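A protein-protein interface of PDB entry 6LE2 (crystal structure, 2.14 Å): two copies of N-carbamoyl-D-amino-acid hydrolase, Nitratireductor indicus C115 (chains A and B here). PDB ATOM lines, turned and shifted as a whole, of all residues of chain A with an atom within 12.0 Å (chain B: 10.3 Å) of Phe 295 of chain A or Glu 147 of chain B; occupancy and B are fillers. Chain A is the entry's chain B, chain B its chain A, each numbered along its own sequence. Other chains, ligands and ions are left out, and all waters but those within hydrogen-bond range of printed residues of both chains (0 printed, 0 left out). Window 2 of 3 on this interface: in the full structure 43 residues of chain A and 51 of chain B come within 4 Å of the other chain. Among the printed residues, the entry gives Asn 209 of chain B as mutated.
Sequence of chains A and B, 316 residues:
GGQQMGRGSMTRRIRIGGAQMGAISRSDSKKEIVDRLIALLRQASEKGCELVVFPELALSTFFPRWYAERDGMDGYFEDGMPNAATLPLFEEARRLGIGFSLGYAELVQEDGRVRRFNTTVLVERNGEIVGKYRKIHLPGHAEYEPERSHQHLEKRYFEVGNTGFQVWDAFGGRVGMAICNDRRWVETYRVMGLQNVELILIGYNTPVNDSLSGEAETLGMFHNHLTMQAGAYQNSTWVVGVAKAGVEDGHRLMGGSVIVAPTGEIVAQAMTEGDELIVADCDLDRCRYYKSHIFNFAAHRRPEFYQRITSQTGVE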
ATOM      1  N   ARG A 288     -25.542  23.443   3.805  1.00  0.00           N
ATOM      2  CA  ARG A 288     -24.729  24.657   3.794  1.00  0.00           C
ATOM      3  C   ARG A 288     -23.317  24.349   3.333  1.00  0.00           C
ATOM      4  O   ARG A 288     -22.714  25.118   2.573  1.00  0.00           O
ATOM      5  CB  ARG A 288     -24.687  25.295   5.186  1.00  0.00           C
ATOM      6  CG  ARG A 288     -25.932  26.066   5.588  1.00  0.00           C
ATOM      7  CD  ARG A 288     -25.987  26.298   7.106  1.00  0.00           C
ATOM      8  NE  ARG A 288     -25.335  27.534   7.519  1.00  0.00           N
ATOM      9  CZ  ARG A 288     -24.343  27.603   8.403  1.00  0.00           C
ATOM     10  NH1 ARG A 288     -23.885  26.499   8.982  1.00  0.00           N
ATOM     11  NH2 ARG A 288     -23.814  28.782   8.719  1.00  0.00           N
ATOM     12  N   TYR A 289     -22.786  23.216   3.782  1.00  0.00           N
ATOM     13  CA  TYR A 289     -21.420  22.834   3.467  1.00  0.00           C
ATOM     14  C   TYR A 289     -21.186  22.846   1.959  1.00  0.00           C
ATOM     15  O   TYR A 289     -20.337  23.587   1.459  1.00  0.00           O
ATOM     16  CB  TYR A 289     -21.145  21.461   4.088  1.00  0.00           C
ATOM     17  CG  TYR A 289     -19.795  20.867   3.798  1.00  0.00           C
ATOM     18  CD1 TYR A 289     -18.630  21.464   4.269  1.00  0.00           C
ATOM     19  CD2 TYR A 289     -19.688  19.684   3.080  1.00  0.00           C
ATOM     20  CE1 TYR A 289     -17.393  20.907   4.007  1.00  0.00           C
ATOM     21  CE2 TYR A 289     -18.462  19.120   2.817  1.00  0.00           C
ATOM     22  CZ  TYR A 289     -17.319  19.733   3.278  1.00  0.00           C
ATOM     23  OH  TYR A 289     -16.102  19.159   3.003  1.00  0.00           O
ATOM     24  N   TYR A 290     -21.976  22.074   1.207  1.00  0.00           N
ATOM     25  CA  TYR A 290     -21.718  21.941  -0.225  1.00  0.00           C
ATOM     26  C   TYR A 290     -22.126  23.179  -1.016  1.00  0.00           C
ATOM     27  O   TYR A 290     -21.604  23.391  -2.117  1.00  0.00           O
ATOM     28  CB  TYR A 290     -22.430  20.699  -0.766  1.00  0.00           C
ATOM     29  CG  TYR A 290     -21.991  19.433  -0.073  1.00  0.00           C
ATOM     30  CD1 TYR A 290     -20.714  18.919  -0.280  1.00  0.00           C
ATOM     31  CD2 TYR A 290     -22.840  18.754   0.801  1.00  0.00           C
ATOM     32  CE1 TYR A 290     -20.286  17.755   0.358  1.00  0.00           C
ATOM     33  CE2 TYR A 290     -22.425  17.580   1.443  1.00  0.00           C
ATOM     34  CZ  TYR A 290     -21.140  17.088   1.217  1.00  0.00           C
ATOM     35  OH  TYR A 290     -20.699  15.935   1.840  1.00  0.00           O
ATOM     36  N   LYS A 291     -23.024  24.005  -0.475  1.00  0.00           N
ATOM     37  CA  LYS A 291     -23.508  25.169  -1.214  1.00  0.00           C
ATOM     38  C   LYS A 291     -22.377  26.145  -1.507  1.00  0.00           C
ATOM     39  O   LYS A 291     -22.213  26.598  -2.644  1.00  0.00           O
ATOM     40  CB  LYS A 291     -24.635  25.852  -0.436  1.00  0.00           C
ATOM     41  CG  LYS A 291     -25.978  25.128  -0.535  1.00  0.00           C
ATOM     42  CD  LYS A 291     -26.991  25.666   0.470  1.00  0.00           C
ATOM     43  CE  LYS A 291     -28.269  24.829   0.531  1.00  0.00           C
ATOM     44  NZ  LYS A 291     -29.058  24.880  -0.743  1.00  0.00           N
ATOM     45  N   SER A 292     -21.571  26.463  -0.498  1.00  0.00           N
ATOM     46  CA  SER A 292     -20.457  27.369  -0.712  1.00  0.00           C
ATOM     47  C   SER A 292     -19.450  27.200   0.414  1.00  0.00           C
ATOM     48  O   SER A 292     -19.813  26.911   1.558  1.00  0.00           O
ATOM     49  CB  SER A 292     -20.921  28.828  -0.780  1.00  0.00           C
ATOM     50  OG  SER A 292     -21.170  29.332   0.519  1.00  0.00           O
ATOM     51  N   HIS A 293     -18.182  27.396   0.070  1.00  0.00           N
ATOM     52  CA  HIS A 293     -17.081  27.344   1.018  1.00  0.00           C
ATOM     53  C   HIS A 293     -16.321  28.667   0.998  1.00  0.00           C
ATOM     54  O   HIS A 293     -16.412  29.435   0.037  1.00  0.00           O
ATOM     55  CB  HIS A 293     -16.137  26.180   0.695  1.00  0.00           C
ATOM     56  CG  HIS A 293     -16.781  24.835   0.814  1.00  0.00           C
ATOM     57  ND1 HIS A 293     -17.114  24.067  -0.283  1.00  0.00           N
ATOM     58  CD2 HIS A 293     -17.164  24.123   1.902  1.00  0.00           C
ATOM     59  CE1 HIS A 293     -17.663  22.938   0.125  1.00  0.00           C
ATOM     60  NE2 HIS A 293     -17.712  22.949   1.445  1.00  0.00           N
ATOM     61  N   ILE A 294     -15.578  28.936   2.079  1.00  0.00           N
ATOM     62  CA  ILE A 294     -14.752  30.147   2.136  1.00  0.00           C
ATOM     63  C   ILE A 294     -13.627  30.080   1.103  1.00  0.00           C
ATOM     64  O   ILE A 294     -13.314  31.077   0.443  1.00  0.00           O
ATOM     65  CB  ILE A 294     -14.210  30.370   3.564  1.00  0.00           C
ATOM     66  CG1 ILE A 294     -15.361  30.562   4.562  1.00  0.00           C
ATOM     67  CG2 ILE A 294     -13.240  31.553   3.604  1.00  0.00           C
ATOM     68  CD1 ILE A 294     -16.349  31.656   4.178  1.00  0.00           C
ATOM     69  N   PHE A 295     -13.003  28.911   0.949  1.00  0.00           N
ATOM     70  CA  PHE A 295     -12.142  28.599  -0.193  1.00  0.00           C
ATOM     71  C   PHE A 295     -12.912  27.646  -1.110  1.00  0.00           C
ATOM     72  O   PHE A 295     -12.731  26.429  -1.052  1.00  0.00           O
ATOM     73  CB  PHE A 295     -10.812  27.952   0.256  1.00  0.00           C
ATOM     74  CG  PHE A 295      -9.943  28.835   1.102  1.00  0.00           C
ATOM     75  CD1 PHE A 295     -10.138  28.913   2.474  1.00  0.00           C
ATOM     76  CD2 PHE A 295      -8.904  29.556   0.532  1.00  0.00           C
ATOM     77  CE1 PHE A 295      -9.328  29.713   3.261  1.00  0.00           C
ATOM     78  CE2 PHE A 295      -8.083  30.360   1.325  1.00  0.00           C
ATOM     79  CZ  PHE A 295      -8.302  30.436   2.683  1.00  0.00           C
ATOM     80  N   ASN A 296     -13.776  28.187  -1.967  1.00  0.00           N
ATOM     81  CA  ASN A 296     -14.549  27.284  -2.816  1.00  0.00           C
ATOM     82  C   ASN A 296     -14.061  27.333  -4.264  1.00  0.00           C
ATOM     83  O   ASN A 296     -13.134  28.068  -4.625  1.00  0.00           O
ATOM     84  CB  ASN A 296     -16.062  27.547  -2.714  1.00  0.00           C
ATOM     85  CG  ASN A 296     -16.460  28.950  -3.111  1.00  0.00           C
ATOM     86  OD1 ASN A 296     -15.621  29.781  -3.471  1.00  0.00           O
ATOM     87  ND2 ASN A 296     -17.763  29.225  -3.049  1.00  0.00           N
ATOM     88  N   PHE A 297     -14.711  26.513  -5.089  1.00  0.00           N
ATOM     89  CA  PHE A 297     -14.234  26.132  -6.409  1.00  0.00           C
ATOM     90  C   PHE A 297     -15.345  26.339  -7.430  1.00  0.00           C
ATOM     91  O   PHE A 297     -15.079  26.601  -8.607  1.00  0.00           O
ATOM     92  CB  PHE A 297     -13.762  24.671  -6.363  1.00  0.00           C
ATOM     93  CG  PHE A 297     -13.411  24.075  -7.703  1.00  0.00           C
ATOM     94  CD1 PHE A 297     -14.398  23.532  -8.526  1.00  0.00           C
ATOM     95  CD2 PHE A 297     -12.091  23.997  -8.113  1.00  0.00           C
ATOM     96  CE1 PHE A 297     -14.078  22.964  -9.750  1.00  0.00           C
ATOM     97  CE2 PHE A 297     -11.766  23.426  -9.328  1.00  0.00           C
ATOM     98  CZ  PHE A 297     -12.763  22.911 -10.150  1.00  0.00           C
ATOM     99  N   ALA A 298     -16.594  26.231  -6.980  1.00  0.00           N
ATOM    100  CA  ALA A 298     -17.739  26.380  -7.867  1.00  0.00           C
ATOM    101  C   ALA A 298     -17.823  27.802  -8.407  1.00  0.00           C
ATOM    102  O   ALA A 298     -17.883  28.770  -7.642  1.00  0.00           O
ATOM    103  CB  ALA A 298     -19.029  26.014  -7.130  1.00  0.00           C
ATOM    104  N   ALA A 299     -17.829  27.922  -9.732  1.00  0.00           N
ATOM    105  CA  ALA A 299     -18.088  29.201 -10.370  1.00  0.00           C
ATOM    106  C   ALA A 299     -19.448  29.741  -9.932  1.00  0.00           C
ATOM    107  O   ALA A 299     -20.277  29.045  -9.343  1.00  0.00           O
ATOM    108  CB  ALA A 299     -18.054  29.061 -11.895  1.00  0.00           C
ATOM    109  N   HIS A 300     -19.682  30.997 -10.234  1.00  0.00           N
ATOM    110  CA  HIS A 300     -20.964  31.599  -9.938  1.00  0.00           C
ATOM    111  C   HIS A 300     -21.885  31.486 -11.149  1.00  0.00           C
ATOM    112  O   HIS A 300     -21.437  31.260 -12.278  1.00  0.00           O
ATOM    113  CB  HIS A 300     -20.778  33.054  -9.517  1.00  0.00           C
ATOM    114  CG  HIS A 300     -21.077  33.289  -8.074  1.00  0.00           C
ATOM    115  ND1 HIS A 300     -21.954  34.258  -7.644  1.00  0.00           N
ATOM    116  CD2 HIS A 300     -20.655  32.640  -6.962  1.00  0.00           C
ATOM    117  CE1 HIS A 300     -22.045  34.211  -6.327  1.00  0.00           C
ATOM    118  NE2 HIS A 300     -21.267  33.236  -5.890  1.00  0.00           N
ATOM    119  N   PRO B 139     -14.345  28.045 -13.142  1.00  0.00           N
ATOM    120  CA  PRO B 139     -14.191  27.652 -11.743  1.00  0.00           C
ATOM    121  C   PRO B 139     -12.909  28.222 -11.139  1.00  0.00           C
ATOM    122  O   PRO B 139     -12.032  28.737 -11.834  1.00  0.00           O
ATOM    123  CB  PRO B 139     -14.113  26.127 -11.832  1.00  0.00           C
ATOM    124  CG  PRO B 139     -13.399  25.891 -13.131  1.00  0.00           C
ATOM    125  CD  PRO B 139     -13.808  27.025 -14.058  1.00  0.00           C
ATOM    126  N   GLY B 140     -12.806  28.093  -9.823  1.00  0.00           N
ATOM    127  CA  GLY B 140     -11.548  28.389  -9.171  1.00  0.00           C
ATOM    128  C   GLY B 140     -11.470  29.800  -8.642  1.00  0.00           C
ATOM    129  O   GLY B 140     -12.471  30.347  -8.172  1.00  0.00           O
ATOM    130  N   HIS B 141     -10.288  30.402  -8.718  1.00  0.00           N
ATOM    131  CA  HIS B 141     -10.033  31.683  -8.081  1.00  0.00           C
ATOM    132  C   HIS B 141      -9.029  32.434  -8.940  1.00  0.00           C
ATOM    133  O   HIS B 141      -8.404  31.862  -9.833  1.00  0.00           O
ATOM    134  CB  HIS B 141      -9.530  31.478  -6.647  1.00  0.00           C
ATOM    135  CG  HIS B 141      -8.498  30.398  -6.539  1.00  0.00           C
ATOM    136  ND1 HIS B 141      -7.166  30.661  -6.295  1.00  0.00           N
ATOM    137  CD2 HIS B 141      -8.596  29.055  -6.696  1.00  0.00           C
ATOM    138  CE1 HIS B 141      -6.493  29.521  -6.285  1.00  0.00           C
ATOM    139  NE2 HIS B 141      -7.336  28.533  -6.533  1.00  0.00           N
ATOM    140  N   ALA B 142      -8.861  33.728  -8.652  1.00  0.00           N
ATOM    141  CA  ALA B 142      -8.085  34.594  -9.533  1.00  0.00           C
ATOM    142  C   ALA B 142      -6.666  34.857  -9.050  1.00  0.00           C
ATOM    143  O   ALA B 142      -5.825  35.276  -9.853  1.00  0.00           O
ATOM    144  CB  ALA B 142      -8.798  35.940  -9.716  1.00  0.00           C
ATOM    145  N   GLU B 143      -6.378  34.651  -7.773  1.00  0.00           N
ATOM    146  CA  GLU B 143      -5.053  34.920  -7.235  1.00  0.00           C
ATOM    147  C   GLU B 143      -4.580  33.742  -6.400  1.00  0.00           C
ATOM    148  O   GLU B 143      -5.371  32.913  -5.936  1.00  0.00           O
ATOM    149  CB  GLU B 143      -5.011  36.204  -6.389  1.00  0.00           C
ATOM    150  CG  GLU B 143      -4.557  37.422  -7.178  1.00  0.00           C
ATOM    151  CD  GLU B 143      -3.073  37.378  -7.534  1.00  0.00           C
ATOM    152  OE1 GLU B 143      -2.326  36.599  -6.885  1.00  0.00           O
ATOM    153  OE2 GLU B 143      -2.660  38.122  -8.459  1.00  0.00           O
ATOM    154  N   TYR B 144      -3.261  33.689  -6.224  1.00  0.00           N
ATOM    155  CA  TYR B 144      -2.630  32.603  -5.491  1.00  0.00           C
ATOM    156  C   TYR B 144      -3.193  32.535  -4.079  1.00  0.00           C
ATOM    157  O   TYR B 144      -3.204  33.538  -3.364  1.00  0.00           O
ATOM    158  CB  TYR B 144      -1.118  32.816  -5.459  1.00  0.00           C
ATOM    159  CG  TYR B 144      -0.374  31.642  -4.891  1.00  0.00           C
ATOM    160  CD1 TYR B 144      -0.278  30.460  -5.606  1.00  0.00           C
ATOM    161  CD2 TYR B 144       0.229  31.710  -3.638  1.00  0.00           C
ATOM    162  CE1 TYR B 144       0.396  29.374  -5.094  1.00  0.00           C
ATOM    163  CE2 TYR B 144       0.911  30.625  -3.115  1.00  0.00           C
ATOM    164  CZ  TYR B 144       0.986  29.457  -3.854  1.00  0.00           C
ATOM    165  OH  TYR B 144       1.651  28.359  -3.365  1.00  0.00           O
ATOM    166  N   GLU B 145      -3.691  31.360  -3.686  1.00  0.00           N
ATOM    167  CA  GLU B 145      -4.286  31.173  -2.363  1.00  0.00           C
ATOM    168  C   GLU B 145      -3.527  30.072  -1.630  1.00  0.00           C
ATOM    169  O   GLU B 145      -3.843  28.880  -1.774  1.00  0.00           O
ATOM    170  CB  GLU B 145      -5.785  30.875  -2.479  1.00  0.00           C
ATOM    171  CG  GLU B 145      -6.593  32.086  -2.978  1.00  0.00           C
ATOM    172  CD  GLU B 145      -8.097  31.840  -3.006  1.00  0.00           C
ATOM    173  OE1 GLU B 145      -8.540  30.750  -2.575  1.00  0.00           O
ATOM    174  OE2 GLU B 145      -8.839  32.736  -3.468  1.00  0.00           O
ATOM    175  N   PRO B 146      -2.532  30.429  -0.807  1.00  0.00           N
ATOM    176  CA  PRO B 146      -1.596  29.419  -0.283  1.00  0.00           C
ATOM    177  C   PRO B 146      -2.211  28.448   0.718  1.00  0.00           C
ATOM    178  O   PRO B 146      -1.579  27.431   1.034  1.00  0.00           O
ATOM    179  CB  PRO B 146      -0.495  30.273   0.377  1.00  0.00           C
ATOM    180  CG  PRO B 146      -1.194  31.540   0.766  1.00  0.00           C
ATOM    181  CD  PRO B 146      -2.225  31.784  -0.313  1.00  0.00           C
ATOM    182  N   GLU B 147      -3.405  28.729   1.237  1.00  0.00           N
ATOM    183  CA  GLU B 147      -4.067  27.772   2.112  1.00  0.00           C
ATOM    184  C   GLU B 147      -4.579  26.547   1.351  1.00  0.00           C
ATOM    185  O   GLU B 147      -4.916  25.542   1.978  1.00  0.00           O
ATOM    186  CB  GLU B 147      -5.217  28.455   2.859  1.00  0.00           C
ATOM    187  CG  GLU B 147      -4.825  29.703   3.674  1.00  0.00           C
ATOM    188  CD  GLU B 147      -4.706  30.977   2.828  1.00  0.00           C
ATOM    189  OE1 GLU B 147      -4.712  30.879   1.575  1.00  0.00           O
ATOM    190  OE2 GLU B 147      -4.602  32.078   3.420  1.00  0.00           O
ATOM    191  N   ARG B 148      -4.637  26.597   0.021  1.00  0.00           N
ATOM    192  CA  ARG B 148      -5.174  25.484  -0.762  1.00  0.00           C
ATOM    193  C   ARG B 148      -4.116  24.414  -1.009  1.00  0.00           C
ATOM    194  O   ARG B 148      -2.948  24.720  -1.266  1.00  0.00           O
ATOM    195  CB  ARG B 148      -5.713  25.977  -2.108  1.00  0.00           C
ATOM    196  CG  ARG B 148      -7.028  26.733  -2.050  1.00  0.00           C
ATOM    197  CD  ARG B 148      -7.332  27.354  -3.408  1.00  0.00           C
ATOM    198  NE  ARG B 148      -8.444  28.306  -3.379  1.00  0.00           N
ATOM    199  CZ  ARG B 148      -9.667  28.050  -3.837  1.00  0.00           C
ATOM    200  NH1 ARG B 148      -9.954  26.865  -4.371  1.00  0.00           N
ATOM    201  NH2 ARG B 148     -10.602  28.987  -3.777  1.00  0.00           N
ATOM    202  N   SER B 149      -4.536  23.147  -0.953  1.00  0.00           N
ATOM    203  CA  SER B 149      -3.625  22.061  -1.305  1.00  0.00           C
ATOM    204  C   SER B 149      -3.157  22.186  -2.756  1.00  0.00           C
ATOM    205  O   SER B 149      -1.972  22.001  -3.054  1.00  0.00           O
ATOM    206  CB  SER B 149      -4.295  20.712  -1.047  1.00  0.00           C
ATOM    207  OG  SER B 149      -5.619  20.706  -1.541  1.00  0.00           O
ATOM    208  N   HIS B 150      -4.058  22.524  -3.670  1.00  0.00           N
ATOM    209  CA  HIS B 150      -3.668  22.799  -5.044  1.00  0.00           C
ATOM    210  C   HIS B 150      -4.380  24.053  -5.526  1.00  0.00           C
ATOM    211  O   HIS B 150      -5.483  24.381  -5.076  1.00  0.00           O
ATOM    212  CB  HIS B 150      -3.934  21.601  -6.007  1.00  0.00           C
ATOM    213  CG  HIS B 150      -5.383  21.267  -6.229  1.00  0.00           C
ATOM    214  ND1 HIS B 150      -6.153  21.874  -7.201  1.00  0.00           N
ATOM    215  CD2 HIS B 150      -6.182  20.339  -5.648  1.00  0.00           C
ATOM    216  CE1 HIS B 150      -7.371  21.360  -7.182  1.00  0.00           C
ATOM    217  NE2 HIS B 150      -7.413  20.424  -6.252  1.00  0.00           N
ATOM    218  N   GLN B 151      -3.726  24.766  -6.433  1.00  0.00           N
ATOM    219  CA  GLN B 151      -4.291  25.974  -7.004  1.00  0.00           C
ATOM    220  C   GLN B 151      -5.193  25.632  -8.176  1.00  0.00           C
ATOM    221  O   GLN B 151      -4.964  24.656  -8.899  1.00  0.00           O
ATOM    222  CB  GLN B 151      -3.185  26.913  -7.477  1.00  0.00           C
ATOM    223  CG  GLN B 151      -2.171  27.240  -6.402  1.00  0.00           C
ATOM    224  CD  GLN B 151      -2.786  27.982  -5.247  1.00  0.00           C
ATOM    225  OE1 GLN B 151      -3.546  28.927  -5.446  1.00  0.00           O
ATOM    226  NE2 GLN B 151      -2.476  27.550  -4.029  1.00  0.00           N
ATOM    227  N   HIS B 152      -6.219  26.454  -8.372  1.00  0.00           N
ATOM    228  CA  HIS B 152      -7.072  26.317  -9.551  1.00  0.00           C
ATOM    229  C   HIS B 152      -7.381  27.720 -10.065  1.00  0.00           C
ATOM    230  O   HIS B 152      -8.364  28.342  -9.651  1.00  0.00           O
ATOM    231  CB  HIS B 152      -8.336  25.540  -9.239  1.00  0.00           C
ATOM    232  CG  HIS B 152      -9.020  25.052 -10.464  1.00  0.00           C
ATOM    233  ND1 HIS B 152      -9.100  23.717 -10.782  1.00  0.00           N
ATOM    234  CD2 HIS B 152      -9.599  25.722 -11.488  1.00  0.00           C
ATOM    235  CE1 HIS B 152      -9.727  23.579 -11.935  1.00  0.00           C
ATOM    236  NE2 HIS B 152     -10.036  24.781 -12.388  1.00  0.00           N
ATOM    237  N   ASN B 209      -8.498  15.675  -5.365  1.00  0.00           N
ATOM    238  CA  ASN B 209      -7.652  15.921  -4.202  1.00  0.00           C
ATOM    239  C   ASN B 209      -6.996  14.627  -3.725  1.00  0.00           C
ATOM    240  O   ASN B 209      -7.578  13.543  -3.811  1.00  0.00           O
ATOM    241  CB  ASN B 209      -8.463  16.542  -3.063  1.00  0.00           C
ATOM    242  CG  ASN B 209      -7.839  17.814  -2.537  1.00  0.00           C
ATOM    243  OD1 ASN B 209      -7.256  18.591  -3.297  1.00  0.00           O
ATOM    244  ND2 ASN B 209      -7.942  18.032  -1.227  1.00  0.00           N
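The backbone carbonyl oxygen (O) of Phe 297 of chain A sits at hydrogen-bond distance from the backbone NH (N) of Gly 140 of chain B (3.0 Å). The guanidinium group (NH2) of Arg 148 of chain B is in hydrogen-bond range of the backbone carbonyl oxygen (O) of Asn 296 of chain A.
OE1 of Glu 145 of chain B is in salt-bridge range of NE of Arg 148 of chain B (2.6 Å). The side-chain amide nitrogen (ND2) of Asn 296 of chain A sits close to the backbone carbonyl oxygen (O) of His 293 of chain A (3.4 Å). The backbone NH of His 141 of chain B sits at hydrogen-bond distance from the backbone carbonyl oxygen of His 152 of chain B (3.0 Å). The guanidinium group of Arg 148 of chain B lies close to a ring nitrogen (NE2) of His 141 of chain B (3.4 Å). The side-chain amide nitrogen (NE2) of Gln 151 of chain B sits at hydrogen-bond distance from the backbone carbonyl oxygen (O) of Glu 145 of chain B, 3.0 Å away.
Among the printed residues, merely in contact across the chains: Phe 297 of chain A with His 152 of chain B (3.1 Å), Phe 295 of chain A with Glu 145 of chain B (3.3 Å), Phe 297 of chain A with Pro 139 of chain B (3.4 Å), Phe 295 of chain A with Glu 147 of chain B (3.4 Å) and Phe 295 of chain A with Arg 148 of chain B (3.8 Å).
Printed residues of chain B within 4 Å of Phe 295 of chain A: Glu 145 (3.3 Å), Glu 147 (3.4 Å) and Arg 148 (3.8 Å). Glu 147 of chain B touches just one residue of chain A: Phe 295 (3.4 Å). No residue of chain B comes within 4 Å of Ile 294 of chain A. Asn 296 of chain A touches just one residue of chain B: Arg 148. Glu 145 of chain B touches just one residue of chain A: Phe 295 (3.3 Å). Pro 146 of chain B touches none of the printed residues of chain A. No residue of chain A comes within 4 Å of Ser 149 of chain B. Of the printed residues of chain A, His 152 of chain B touches Phe 297. Printed residues of chain A within 4 Å of Pro 139 of chain B: Phe 297. Of the printed residues of chain B, Phe 297 of chain A touches Pro 139, Gly 140 and His 152. Printed residues of chain A within 4 Å of Gly 140 of chain B: Phe 297. Tyr 144 of chain B touches none of the printed residues of chain A. Gln 151 of chain B touches none of the printed residues of chain A. The nearest residue of chain A that does not touch Glu 147 of chain B is Ile 294 of chain A (8.6 Å). The nearest printed residue of chain A that does not touch Pro 139 of chain B is Ala 299 of chain A (4.04 Å).
Hydrophobic or aromatic side chains of chain A that line the printed part of chain B: Phe 295 and Phe 297. Printed residues of chain B that touch a printed residue of chain A: Pro 139, Gly 140, Glu 145, Glu 147, Arg 148 and His 152. Hydrophobic or aromatic side chains of chain B within 4 Å of the printed part of chain A: Pro 139 and His 152. Among the printed residues, 7 pairs touch across the chains. Among the printed residues, no Asp or Glu carboxylate lies within 4 Å of a Lys or Arg side-chain nitrogen of the other chain.
No position is printed for both chains. Of the 7 pairs that touch across the chains among the printed residues, none has its exchanged pair printed and touching as well.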
